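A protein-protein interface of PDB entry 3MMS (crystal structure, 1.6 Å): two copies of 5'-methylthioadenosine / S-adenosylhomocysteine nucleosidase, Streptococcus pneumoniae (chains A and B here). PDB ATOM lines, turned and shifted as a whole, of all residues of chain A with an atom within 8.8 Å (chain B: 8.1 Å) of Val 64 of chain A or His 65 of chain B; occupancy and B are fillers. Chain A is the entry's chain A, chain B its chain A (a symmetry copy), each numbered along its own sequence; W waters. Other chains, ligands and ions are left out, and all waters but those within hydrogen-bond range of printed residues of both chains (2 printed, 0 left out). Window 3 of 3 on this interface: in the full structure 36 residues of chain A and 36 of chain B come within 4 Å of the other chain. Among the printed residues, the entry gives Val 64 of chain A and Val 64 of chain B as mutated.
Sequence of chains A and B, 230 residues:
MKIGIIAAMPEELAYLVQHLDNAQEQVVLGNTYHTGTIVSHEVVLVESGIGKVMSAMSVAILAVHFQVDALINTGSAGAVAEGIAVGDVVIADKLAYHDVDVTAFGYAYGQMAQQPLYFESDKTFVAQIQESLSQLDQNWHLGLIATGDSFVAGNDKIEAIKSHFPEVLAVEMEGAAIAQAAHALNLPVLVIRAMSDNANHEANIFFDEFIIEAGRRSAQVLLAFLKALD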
ATOM      1  N   VAL A  28     -15.959   6.811  18.100  1.00  0.00           N
ATOM      2  CA  VAL A  28     -15.364   7.802  18.984  1.00  0.00           C
ATOM      3  C   VAL A  28     -14.397   8.694  18.216  1.00  0.00           C
ATOM      4  O   VAL A  28     -13.405   8.218  17.666  1.00  0.00           O
ATOM      5  CB  VAL A  28     -14.619   7.135  20.153  1.00  0.00           C
ATOM      6  CG1 VAL A  28     -14.013   8.187  21.067  1.00  0.00           C
ATOM      7  CG2 VAL A  28     -15.554   6.221  20.928  1.00  0.00           C
ATOM      8  N   LEU A  29     -14.700   9.949  18.154  1.00  0.00           N
ATOM      9  CA  LEU A  29     -13.870  10.883  17.438  1.00  0.00           C
ATOM     10  C   LEU A  29     -13.432  10.422  16.067  1.00  0.00           C
ATOM     11  O   LEU A  29     -12.235  10.358  15.733  1.00  0.00           O
ATOM     12  CB  LEU A  29     -12.650  11.271  18.270  1.00  0.00           C
ATOM     13  CG  LEU A  29     -12.936  11.577  19.729  1.00  0.00           C
ATOM     14  CD1 LEU A  29     -11.635  11.747  20.495  1.00  0.00           C
ATOM     15  CD2 LEU A  29     -13.829  12.797  19.901  1.00  0.00           C
ATOM     16  N   TYR A  33     -14.796   1.646  17.171  1.00  0.00           N
ATOM     17  CA  TYR A  33     -14.301   0.717  18.173  1.00  0.00           C
ATOM     18  C   TYR A  33     -15.308  -0.414  18.260  1.00  0.00           C
ATOM     19  O   TYR A  33     -16.511  -0.166  18.450  1.00  0.00           O
ATOM     20  CB  TYR A  33     -14.165   1.443  19.518  1.00  0.00           C
ATOM     21  CG  TYR A  33     -13.039   2.442  19.516  1.00  0.00           C
ATOM     22  CD1 TYR A  33     -13.178   3.683  18.891  1.00  0.00           C
ATOM     23  CD2 TYR A  33     -11.794   2.120  20.080  1.00  0.00           C
ATOM     24  CE1 TYR A  33     -12.111   4.581  18.820  1.00  0.00           C
ATOM     25  CE2 TYR A  33     -10.720   3.011  20.016  1.00  0.00           C
ATOM     26  CZ  TYR A  33     -10.889   4.238  19.382  1.00  0.00           C
ATOM     27  OH  TYR A  33      -9.818   5.095  19.312  1.00  0.00           O
ATOM     28  N   MET A  57      -2.683   7.327  19.821  1.00  0.00           N
ATOM     29  CA  MET A  57      -4.026   7.808  20.122  1.00  0.00           C
ATOM     30  C   MET A  57      -4.961   6.660  20.451  1.00  0.00           C
ATOM     31  O   MET A  57      -5.794   6.777  21.354  1.00  0.00           O
ATOM     32  CB  MET A  57      -4.616   8.603  18.952  1.00  0.00           C
ATOM     33  CG  MET A  57      -3.926   9.922  18.750  1.00  0.00           C
ATOM     34  SD  MET A  57      -4.951  10.954  17.641  1.00  0.00           S
ATOM     35  CE  MET A  57      -4.794  10.061  16.172  1.00  0.00           C
ATOM     36  N   SER A  58      -4.904   5.492  19.715  1.00  0.00           N
ATOM     37  CA  SER A  58      -5.783   4.372  20.030  1.00  0.00           C
ATOM     38  C   SER A  58      -5.511   3.836  21.434  1.00  0.00           C
ATOM     39  O   SER A  58      -6.441   3.531  22.164  1.00  0.00           O
ATOM     40  CB  SER A  58      -5.621   3.253  18.999  1.00  0.00           C
ATOM     41  OG  SER A  58      -5.892   3.726  17.691  1.00  0.00           O
ATOM     42  N   VAL A  59      -4.218   3.778  21.813  1.00  0.00           N
ATOM     43  CA  VAL A  59      -3.945   3.268  23.148  1.00  0.00           C
ATOM     44  C   VAL A  59      -4.566   4.200  24.184  1.00  0.00           C
ATOM     45  O   VAL A  59      -5.215   3.738  25.136  1.00  0.00           O
ATOM     46  CB  VAL A  59      -2.440   3.143  23.407  1.00  0.00           C
ATOM     47  CG1 VAL A  59      -2.173   2.829  24.881  1.00  0.00           C
ATOM     48  CG2 VAL A  59      -1.885   2.060  22.518  1.00  0.00           C
ATOM     49  N   ALA A  60      -4.378   5.505  24.000  1.00  0.00           N
ATOM     50  CA  ALA A  60      -4.912   6.471  24.955  1.00  0.00           C
ATOM     51  C   ALA A  60      -6.433   6.377  25.058  1.00  0.00           C
ATOM     52  O   ALA A  60      -6.987   6.447  26.155  1.00  0.00           O
ATOM     53  CB  ALA A  60      -4.482   7.890  24.571  1.00  0.00           C
ATOM     54  N   ILE A  61      -7.116   6.218  23.925  1.00  0.00           N
ATOM     55  CA  ILE A  61      -8.588   6.148  23.968  1.00  0.00           C
ATOM     56  C   ILE A  61      -9.059   4.826  24.560  1.00  0.00           C
ATOM     57  O   ILE A  61     -10.023   4.804  25.323  1.00  0.00           O
ATOM     58  CB  ILE A  61      -9.171   6.398  22.557  1.00  0.00           C
ATOM     59  CG1 ILE A  61      -8.886   7.852  22.178  1.00  0.00           C
ATOM     60  CG2 ILE A  61     -10.690   6.074  22.519  1.00  0.00           C
ATOM     61  CD1 ILE A  61      -9.072   8.178  20.697  1.00  0.00           C
ATOM     62  N   LEU A  62      -8.386   3.733  24.226  1.00  0.00           N
ATOM     63  CA  LEU A  62      -8.701   2.448  24.839  1.00  0.00           C
ATOM     64  C   LEU A  62      -8.535   2.512  26.355  1.00  0.00           C
ATOM     65  O   LEU A  62      -9.357   1.982  27.101  1.00  0.00           O
ATOM     66  CB  LEU A  62      -7.827   1.338  24.255  1.00  0.00           C
ATOM     67  CG  LEU A  62      -8.198   0.881  22.844  1.00  0.00           C
ATOM     68  CD1 LEU A  62      -7.139  -0.054  22.289  1.00  0.00           C
ATOM     69  CD2 LEU A  62      -9.563   0.217  22.836  1.00  0.00           C
ATOM     70  N   ALA A  63      -7.473   3.173  26.802  1.00  0.00           N
ATOM     71  CA  ALA A  63      -7.193   3.289  28.228  1.00  0.00           C
ATOM     72  C   ALA A  63      -8.210   4.183  28.928  1.00  0.00           C
ATOM     73  O   ALA A  63      -8.812   3.789  29.925  1.00  0.00           O
ATOM     74  CB  ALA A  63      -5.781   3.809  28.452  1.00  0.00           C
ATOM     75  N   VAL A  64      -8.395   5.391  28.405  1.00  0.00           N
ATOM     76  CA  VAL A  64      -9.124   6.427  29.127  1.00  0.00           C
ATOM     77  C   VAL A  64     -10.632   6.278  28.959  1.00  0.00           C
ATOM     78  O   VAL A  64     -11.391   6.466  29.908  1.00  0.00           O
ATOM     79  CB  VAL A  64      -8.698   7.842  28.690  1.00  0.00           C
ATOM     80  CG1 VAL A  64      -9.320   8.197  27.350  1.00  0.00           C
ATOM     81  CG2 VAL A  64      -9.092   8.863  29.745  1.00  0.00           C
ATOM     82  N   HIS A  65     -11.063   5.943  27.747  1.00  0.00           N
ATOM     83  CA  HIS A  65     -12.486   5.875  27.445  1.00  0.00           C
ATOM     84  C   HIS A  65     -13.063   4.487  27.694  1.00  0.00           C
ATOM     85  O   HIS A  65     -14.117   4.351  28.314  1.00  0.00           O
ATOM     86  CB  HIS A  65     -12.766   6.313  26.008  1.00  0.00           C
ATOM     87  CG  HIS A  65     -14.224   6.419  25.687  1.00  0.00           C
ATOM     88  ND1 HIS A  65     -15.008   7.464  26.128  1.00  0.00           N
ATOM     89  CD2 HIS A  65     -15.043   5.608  24.977  1.00  0.00           C
ATOM     90  CE1 HIS A  65     -16.245   7.294  25.700  1.00  0.00           C
ATOM     91  NE2 HIS A  65     -16.294   6.175  24.999  1.00  0.00           N
ATOM     92  N   PHE A  66     -12.376   3.458  27.211  1.00  0.00           N
ATOM     93  CA  PHE A  66     -12.872   2.095  27.364  1.00  0.00           C
ATOM     94  C   PHE A  66     -12.371   1.408  28.619  1.00  0.00           C
ATOM     95  O   PHE A  66     -12.835   0.316  28.961  1.00  0.00           O
ATOM     96  CB  PHE A  66     -12.533   1.275  26.110  1.00  0.00           C
ATOM     97  CG  PHE A  66     -13.305   1.712  24.883  1.00  0.00           C
ATOM     98  CD1 PHE A  66     -14.592   1.230  24.647  1.00  0.00           C
ATOM     99  CD2 PHE A  66     -12.768   2.659  24.001  1.00  0.00           C
ATOM    100  CE1 PHE A  66     -15.336   1.687  23.548  1.00  0.00           C
ATOM    101  CE2 PHE A  66     -13.502   3.126  22.901  1.00  0.00           C
ATOM    102  CZ  PHE A  66     -14.800   2.636  22.672  1.00  0.00           C
ATOM    103  N   GLN A  67     -11.430   2.052  29.311  1.00  0.00           N
ATOM    104  CA  GLN A  67     -10.896   1.498  30.553  1.00  0.00           C
ATOM    105  C   GLN A  67     -10.423   0.051  30.439  1.00  0.00           C
ATOM    106  O   GLN A  67     -10.701  -0.802  31.297  1.00  0.00           O
ATOM    107  CB  GLN A  67     -11.950   1.649  31.666  1.00  0.00           C
ATOM    108  CG  GLN A  67     -12.269   3.125  31.902  1.00  0.00           C
ATOM    109  CD  GLN A  67     -13.213   3.378  33.056  1.00  0.00           C
ATOM    110  OE1 GLN A  67     -14.289   2.783  33.135  1.00  0.00           O
ATOM    111  NE2 GLN A  67     -12.822   4.277  33.954  1.00  0.00           N
ATOM    112  N   VAL A  68      -9.675  -0.235  29.381  1.00  0.00           N
ATOM    113  CA  VAL A  68      -9.157  -1.587  29.226  1.00  0.00           C
ATOM    114  C   VAL A  68      -8.069  -1.882  30.273  1.00  0.00           C
ATOM    115  O   VAL A  68      -7.485  -0.956  30.877  1.00  0.00           O
ATOM    116  CB  VAL A  68      -8.584  -1.824  27.793  1.00  0.00           C
ATOM    117  CG1 VAL A  68      -9.679  -1.527  26.746  1.00  0.00           C
ATOM    118  CG2 VAL A  68      -7.355  -0.932  27.545  1.00  0.00           C
ATOM    119  N   LEU A  71      -3.526  -4.782  26.613  1.00  0.00           N
ATOM    120  CA  LEU A  71      -3.530  -4.550  25.185  1.00  0.00           C
ATOM    121  C   LEU A  71      -2.831  -5.667  24.408  1.00  0.00           C
ATOM    122  O   LEU A  71      -1.859  -6.273  24.891  1.00  0.00           O
ATOM    123  CB  LEU A  71      -2.806  -3.244  24.916  1.00  0.00           C
ATOM    124  CG  LEU A  71      -3.435  -2.000  25.535  1.00  0.00           C
ATOM    125  CD1 LEU A  71      -2.433  -0.850  25.546  1.00  0.00           C
ATOM    126  CD2 LEU A  71      -4.667  -1.618  24.715  1.00  0.00           C
ATOM    127  N   LEU A 185       0.768   4.558  30.302  1.00  0.00           N
ATOM    128  CA  LEU A 185      -0.577   4.483  30.857  1.00  0.00           C
ATOM    129  C   LEU A 185      -0.771   3.290  31.768  1.00  0.00           C
ATOM    130  O   LEU A 185      -1.901   2.941  32.125  1.00  0.00           O
ATOM    131  CB  LEU A 185      -1.608   4.476  29.726  1.00  0.00           C
ATOM    132  CG  LEU A 185      -1.468   5.668  28.762  1.00  0.00           C
ATOM    133  CD1 LEU A 185      -2.605   5.607  27.713  1.00  0.00           C
ATOM    134  CD2 LEU A 185      -1.511   7.000  29.535  1.00  0.00           C
ATOM    135  N   LEU A 187      -0.285  -0.086  31.385  1.00  0.00           N
ATOM    136  CA  LEU A 187      -1.008  -1.242  30.860  1.00  0.00           C
ATOM    137  C   LEU A 187      -0.062  -2.258  30.260  1.00  0.00           C
ATOM    138  O   LEU A 187       0.900  -1.885  29.598  1.00  0.00           O
ATOM    139  CB  LEU A 187      -1.997  -0.823  29.765  1.00  0.00           C
ATOM    140  CG  LEU A 187      -3.196   0.018  30.186  1.00  0.00           C
ATOM    141  CD1 LEU A 187      -3.873   0.583  28.935  1.00  0.00           C
ATOM    142  CD2 LEU A 187      -4.162  -0.818  31.018  1.00  0.00           C
ATOM    143  N   LYS B   2     -13.591  25.700  24.821  1.00  0.00           N
ATOM    144  CA  LYS B   2     -12.704  25.103  25.913  1.00  0.00           C
ATOM    145  C   LYS B   2     -11.371  24.715  25.121  1.00  0.00           C
ATOM    146  O   LYS B   2     -11.361  23.895  24.206  1.00  0.00           O
ATOM    147  CB  LYS B   2     -13.325  23.881  26.439  1.00  0.00           C
ATOM    148  CG  LYS B   2     -12.516  23.263  27.565  1.00  0.00           C
ATOM    149  CD  LYS B   2     -13.070  21.901  27.947  1.00  0.00           C
ATOM    150  CE  LYS B   2     -12.868  21.613  29.423  1.00  0.00           C
ATOM    151  NZ  LYS B   2     -13.683  20.455  29.881  1.00  0.00           N
ATOM    152  N   GLN B  26      -6.051  17.489  37.906  1.00  0.00           N
ATOM    153  CA  GLN B  26      -6.767  16.239  37.788  1.00  0.00           C
ATOM    154  C   GLN B  26      -5.761  15.258  37.221  1.00  0.00           C
ATOM    155  O   GLN B  26      -5.170  15.513  36.165  1.00  0.00           O
ATOM    156  CB  GLN B  26      -7.951  16.448  36.842  1.00  0.00           C
ATOM    157  CG  GLN B  26      -8.851  15.270  36.634  1.00  0.00           C
ATOM    158  CD  GLN B  26     -10.109  15.662  35.873  1.00  0.00           C
ATOM    159  OE1 GLN B  26     -10.821  14.804  35.339  1.00  0.00           O
ATOM    160  NE2 GLN B  26     -10.396  16.969  35.832  1.00  0.00           N
ATOM    161  N   VAL B  27      -5.531  14.161  37.929  1.00  0.00           N
ATOM    162  CA  VAL B  27      -4.587  13.159  37.460  1.00  0.00           C
ATOM    163  C   VAL B  27      -5.311  12.107  36.641  1.00  0.00           C
ATOM    164  O   VAL B  27      -6.226  11.437  37.124  1.00  0.00           O
ATOM    165  CB  VAL B  27      -3.868  12.472  38.625  1.00  0.00           C
ATOM    166  CG1 VAL B  27      -2.974  11.369  38.105  1.00  0.00           C
ATOM    167  CG2 VAL B  27      -3.059  13.499  39.391  1.00  0.00           C
ATOM    168  N   VAL B  28      -4.898  11.972  35.386  1.00  0.00           N
ATOM    169  CA  VAL B  28      -5.471  10.980  34.487  1.00  0.00           C
ATOM    170  C   VAL B  28      -4.389  10.050  33.955  1.00  0.00           C
ATOM    171  O   VAL B  28      -3.456  10.489  33.284  1.00  0.00           O
ATOM    172  CB  VAL B  28      -6.193  11.647  33.303  1.00  0.00           C
ATOM    173  CG1 VAL B  28      -6.790  10.595  32.384  1.00  0.00           C
ATOM    174  CG2 VAL B  28      -7.268  12.599  33.803  1.00  0.00           C
ATOM    175  N   LEU B  29      -4.495   8.803  34.277  1.00  0.00           N
ATOM    176  CA  LEU B  29      -3.519   7.835  33.848  1.00  0.00           C
ATOM    177  C   LEU B  29      -2.081   8.261  34.028  1.00  0.00           C
ATOM    178  O   LEU B  29      -1.267   8.286  33.087  1.00  0.00           O
ATOM    179  CB  LEU B  29      -3.763   7.429  32.396  1.00  0.00           C
ATOM    180  CG  LEU B  29      -5.213   7.155  32.038  1.00  0.00           C
ATOM    181  CD1 LEU B  29      -5.356   6.963  30.538  1.00  0.00           C
ATOM    182  CD2 LEU B  29      -5.781   5.963  32.793  1.00  0.00           C
ATOM    183  N   TYR B  33      -3.424  17.088  34.641  1.00  0.00           N
ATOM    184  CA  TYR B  33      -4.095  18.020  33.751  1.00  0.00           C
ATOM    185  C   TYR B  33      -4.572  19.179  34.606  1.00  0.00           C
ATOM    186  O   TYR B  33      -5.262  18.966  35.617  1.00  0.00           O
ATOM    187  CB  TYR B  33      -5.273  17.314  33.067  1.00  0.00           C
ATOM    188  CG  TYR B  33      -4.818  16.285  32.067  1.00  0.00           C
ATOM    189  CD1 TYR B  33      -4.346  15.037  32.480  1.00  0.00           C
ATOM    190  CD2 TYR B  33      -4.789  16.583  30.695  1.00  0.00           C
ATOM    191  CE1 TYR B  33      -3.851  14.109  31.560  1.00  0.00           C
ATOM    192  CE2 TYR B  33      -4.298  15.662  29.766  1.00  0.00           C
ATOM    193  CZ  TYR B  33      -3.830  14.429  30.210  1.00  0.00           C
ATOM    194  OH  TYR B  33      -3.333  13.543  29.285  1.00  0.00           O
ATOM    195  N   VAL B  44      -7.553  23.595  29.541  1.00  0.00           N
ATOM    196  CA  VAL B  44      -6.887  22.496  30.225  1.00  0.00           C
ATOM    197  C   VAL B  44      -5.421  22.455  29.815  1.00  0.00           C
ATOM    198  O   VAL B  44      -5.106  22.371  28.630  1.00  0.00           O
ATOM    199  CB  VAL B  44      -7.532  21.144  29.867  1.00  0.00           C
ATOM    200  CG1 VAL B  44      -6.975  20.032  30.743  1.00  0.00           C
ATOM    201  CG2 VAL B  44      -9.044  21.226  29.989  1.00  0.00           C
ATOM    202  N   MET B  57      -0.815  11.129  22.654  1.00  0.00           N
ATOM    203  CA  MET B  57      -1.672  10.690  23.748  1.00  0.00           C
ATOM    204  C   MET B  57      -2.337  11.868  24.434  1.00  0.00           C
ATOM    205  O   MET B  57      -3.511  11.789  24.804  1.00  0.00           O
ATOM    206  CB  MET B  57      -0.886   9.891  24.795  1.00  0.00           C
ATOM    207  CG  MET B  57      -0.445   8.551  24.278  1.00  0.00           C
ATOM    208  SD  MET B  57       0.093   7.528  25.696  1.00  0.00           S
ATOM    209  CE  MET B  57       1.513   8.391  26.166  1.00  0.00           C
ATOM    210  N   SER B  58      -1.615  13.021  24.676  1.00  0.00           N
ATOM    211  CA  SER B  58      -2.245  14.169  25.318  1.00  0.00           C
ATOM    212  C   SER B  58      -3.384  14.722  24.464  1.00  0.00           C
ATOM    213  O   SER B  58      -4.432  15.064  24.989  1.00  0.00           O
ATOM    214  CB  SER B  58      -1.213  15.266  25.592  1.00  0.00           C
ATOM    215  OG  SER B  58      -0.159  14.779  26.403  1.00  0.00           O
ATOM    216  N   VAL B  59      -3.174  14.752  23.132  1.00  0.00           N
ATOM    217  CA  VAL B  59      -4.252  15.277  22.308  1.00  0.00           C
ATOM    218  C   VAL B  59      -5.479  14.380  22.443  1.00  0.00           C
ATOM    219  O   VAL B  59      -6.603  14.875  22.616  1.00  0.00           O
ATOM    220  CB  VAL B  59      -3.842  15.366  20.834  1.00  0.00           C
ATOM    221  CG1 VAL B  59      -5.053  15.697  19.959  1.00  0.00           C
ATOM    222  CG2 VAL B  59      -2.772  16.418  20.693  1.00  0.00           C
ATOM    223  N   ALA B  60      -5.267  13.067  22.374  1.00  0.00           N
ATOM    224  CA  ALA B  60      -6.384  12.132  22.466  1.00  0.00           C
ATOM    225  C   ALA B  60      -7.122  12.268  23.797  1.00  0.00           C
ATOM    226  O   ALA B  60      -8.352  12.233  23.831  1.00  0.00           O
ATOM    227  CB  ALA B  60      -5.892  10.695  22.266  1.00  0.00           C
ATOM    228  N   ILE B  61      -6.384  12.427  24.894  1.00  0.00           N
ATOM    229  CA  ILE B  61      -7.048  12.537  26.206  1.00  0.00           C
ATOM    230  C   ILE B  61      -7.749  13.881  26.357  1.00  0.00           C
ATOM    231  O   ILE B  61      -8.849  13.942  26.903  1.00  0.00           O
ATOM    232  CB  ILE B  61      -6.027  12.278  27.339  1.00  0.00           C
ATOM    233  CG1 ILE B  61      -5.602  10.811  27.267  1.00  0.00           C
ATOM    234  CG2 ILE B  61      -6.631  12.642  28.724  1.00  0.00           C
ATOM    235  CD1 ILE B  61      -4.350  10.465  28.073  1.00  0.00           C
ATOM    236  N   LEU B  62      -7.131  14.950  25.872  1.00  0.00           N
ATOM    237  CA  LEU B  62      -7.785  16.252  25.873  1.00  0.00           C
ATOM    238  C   LEU B  62      -9.087  16.210  25.078  1.00  0.00           C
ATOM    239  O   LEU B  62     -10.097  16.774  25.495  1.00  0.00           O
ATOM    240  CB  LEU B  62      -6.855  17.328  25.313  1.00  0.00           C
ATOM    241  CG  LEU B  62      -5.724  17.771  26.243  1.00  0.00           C
ATOM    242  CD1 LEU B  62      -4.746  18.668  25.506  1.00  0.00           C
ATOM    243  CD2 LEU B  62      -6.281  18.471  27.469  1.00  0.00           C
ATOM    244  N   ALA B  63      -9.056  15.528  23.939  1.00  0.00           N
ATOM    245  CA  ALA B  63     -10.230  15.429  23.080  1.00  0.00           C
ATOM    246  C   ALA B  63     -11.321  14.575  23.715  1.00  0.00           C
ATOM    247  O   ALA B  63     -12.468  15.002  23.828  1.00  0.00           O
ATOM    248  CB  ALA B  63      -9.845  14.876  21.715  1.00  0.00           C
ATOM    249  N   VAL B  64     -10.958  13.364  24.126  1.00  0.00           N
ATOM    250  CA  VAL B  64     -11.950  12.360  24.496  1.00  0.00           C
ATOM    251  C   VAL B  64     -12.436  12.546  25.929  1.00  0.00           C
ATOM    252  O   VAL B  64     -13.623  12.395  26.213  1.00  0.00           O
ATOM    253  CB  VAL B  64     -11.411  10.927  24.321  1.00  0.00           C
ATOM    254  CG1 VAL B  64     -10.474  10.566  25.461  1.00  0.00           C
ATOM    255  CG2 VAL B  64     -12.561   9.935  24.245  1.00  0.00           C
ATOM    256  N   HIS B  65     -11.514  12.872  26.829  1.00  0.00           N
ATOM    257  CA  HIS B  65     -11.846  12.974  28.244  1.00  0.00           C
ATOM    258  C   HIS B  65     -12.280  14.380  28.636  1.00  0.00           C
ATOM    259  O   HIS B  65     -13.285  14.556  29.322  1.00  0.00           O
ATOM    260  CB  HIS B  65     -10.677  12.518  29.117  1.00  0.00           C
ATOM    261  CG  HIS B  65     -11.011  12.446  30.575  1.00  0.00           C
ATOM    262  ND1 HIS B  65     -11.771  11.431  31.113  1.00  0.00           N
ATOM    263  CD2 HIS B  65     -10.696  13.267  31.604  1.00  0.00           C
ATOM    264  CE1 HIS B  65     -11.906  11.627  32.412  1.00  0.00           C
ATOM    265  NE2 HIS B  65     -11.263  12.734  32.736  1.00  0.00           N
ATOM    266  N   PHE B  66     -11.522  15.382  28.203  1.00  0.00           N
ATOM    267  CA  PHE B  66     -11.835  16.760  28.563  1.00  0.00           C
ATOM    268  C   PHE B  66     -12.739  17.455  27.564  1.00  0.00           C
ATOM    269  O   PHE B  66     -13.216  18.565  27.818  1.00  0.00           O
ATOM    270  CB  PHE B  66     -10.535  17.549  28.777  1.00  0.00           C
ATOM    271  CG  PHE B  66      -9.765  17.113  30.006  1.00  0.00           C
ATOM    272  CD1 PHE B  66     -10.087  17.625  31.263  1.00  0.00           C
ATOM    273  CD2 PHE B  66      -8.765  16.136  29.913  1.00  0.00           C
ATOM    274  CE1 PHE B  66      -9.422  17.169  32.412  1.00  0.00           C
ATOM    275  CE2 PHE B  66      -8.095  15.671  31.054  1.00  0.00           C
ATOM    276  CZ  PHE B  66      -8.427  16.191  32.317  1.00  0.00           C
ATOM    277  N   GLN B  67     -12.981  16.798  26.428  1.00  0.00           N
ATOM    278  CA  GLN B  67     -13.862  17.359  25.406  1.00  0.00           C
ATOM    279  C   GLN B  67     -13.519  18.790  25.002  1.00  0.00           C
ATOM    280  O   GLN B  67     -14.390  19.664  24.874  1.00  0.00           O
ATOM    281  CB  GLN B  67     -15.322  17.255  25.887  1.00  0.00           C
ATOM    282  CG  GLN B  67     -15.710  15.792  26.100  1.00  0.00           C
ATOM    283  CD  GLN B  67     -17.162  15.585  26.466  1.00  0.00           C
ATOM    284  OE1 GLN B  67     -17.676  16.209  27.396  1.00  0.00           O
ATOM    285  NE2 GLN B  67     -17.832  14.690  25.745  1.00  0.00           N
ATOM    286  N   VAL B  68     -12.235  19.038  24.772  1.00  0.00           N
ATOM    287  CA  VAL B  68     -11.838  20.372  24.347  1.00  0.00           C
ATOM    288  C   VAL B  68     -12.314  20.656  22.912  1.00  0.00           C
ATOM    289  O   VAL B  68     -12.636  19.725  22.142  1.00  0.00           O
ATOM    290  CB  VAL B  68     -10.292  20.569  24.436  1.00  0.00           C
ATOM    291  CG1 VAL B  68      -9.819  20.285  25.877  1.00  0.00           C
ATOM    292  CG2 VAL B  68      -9.568  19.640  23.445  1.00  0.00           C
HETATM  293  O   HOH W   1     -14.409   9.527  27.696  1.00  0.00           O
HETATM  294  O   HOH W   2     -12.990   9.380  29.938  1.00  0.00           O
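Water W1 bridges ND1 of His 65 of chain A and O of Val 64 of chain B. Water W2 bridges a ring nitrogen (ND1) of His 65 of chain B and the backbone carbonyl oxygen of Val 64 of chain A.
Printed residues of chain B that touch a printed residue of chain A: Val 28, Leu 29, Met 57, Ala 60, Ala 63, Val 64 and His 65. Hydrophobic or aromatic side chains of chain B that line the printed part of chain A: Val 28, Leu 29, Met 57, Ala 60, Ala 63, Val 64 and His 65. Of the 18 printed residues of chain A, 7 touch a printed residue of chain B. Printed residues of chain A that touch a printed residue of chain B: Val 28, Leu 29, Ala 60, Ala 63, Val 64, His 65 and Leu 185. Among the printed residues, 12 pairs touch across the chains.
NE2 of His 65 of chain B sits at hydrogen-bond distance from OE1 of Gln 26 of chain B.
CG1 of Val 28 of chain A touches CG2 of Val 64 of chain B (3.9 Å). Val 64 of chain B touches Leu 29 of chain A (CB to CD1, 3.9 Å). CB of Ala 63 of chain A touches CD1 of Leu 29 of chain B (3.8 Å). CG1 of Val 28 of chain B touches CG2 of Val 64 of chain A, at 3.9 Å. CD1 of Leu 29 of chain B touches CB of Val 64 of chain A, at 3.9 Å. Val 64 of chain B touches Val 64 of chain A. CG2 of Val 64 of chain A touches ND1 of His 65 of chain B (3.96 Å). ND1 of His 65 of chain A touches CG2 of Val 64 of chain B, at 3.95 Å. Leu 29 of chain B touches Leu 185 of chain A (CB to CD2, 3.7 Å). Leu 185 of chain A touches Met 57 of chain B (CD1 to SD, 3.9 Å).
Leu 29 of chain A touches Ala 63 of chain B, and with the chains exchanged Ala 63 of chain A touches Leu 29 of chain B. Ala 60 of chain B touches its own counterpart, Ala 60 of chain A. Val 64 of chain A touches its own counterpart, Val 64 of chain B. Val 64 of chain A touches His 65 of chain B, and with the chains exchanged His 65 of chain A touches Val 64 of chain B. Positions printed for both chains: 28, 29, 33, 57, 58, 59, 60, 61, 62, 63, 64, 65, 66, 67 and 68. Of the 12 pairs that touch across the chains among the printed residues, 10 have their exchanged pair printed and touching as well.
His 65 of chain B touches one residue of chain A. Ala 63 of chain A touches one residue of chain B. No residue of chain A comes within 4 Å of Phe 66 of chain B. Printed residues of chain A within 4 Å of Ala 60 of chain B: Ala 60. Printed residues of chain B within 4 Å of Val 28 of chain A: Val 64. Of the printed residues of chain A, Met 57 of chain B touches Leu 185. Of the printed residues of chain A, Val 28 of chain B touches Val 64. Val 59 of chain A touches none of the printed residues of chain B. The nearest residue of chain B that does not touch Val 64 of chain A is Ile 61 of chain B (4.5 Å). The nearest residue of chain A that does not touch His 65 of chain B is Leu 29 of chain A (6.4 Å). The nearest printed residue of chain A that does not touch Ala 60 of chain B is Met 57 of chain A (4.02 Å).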
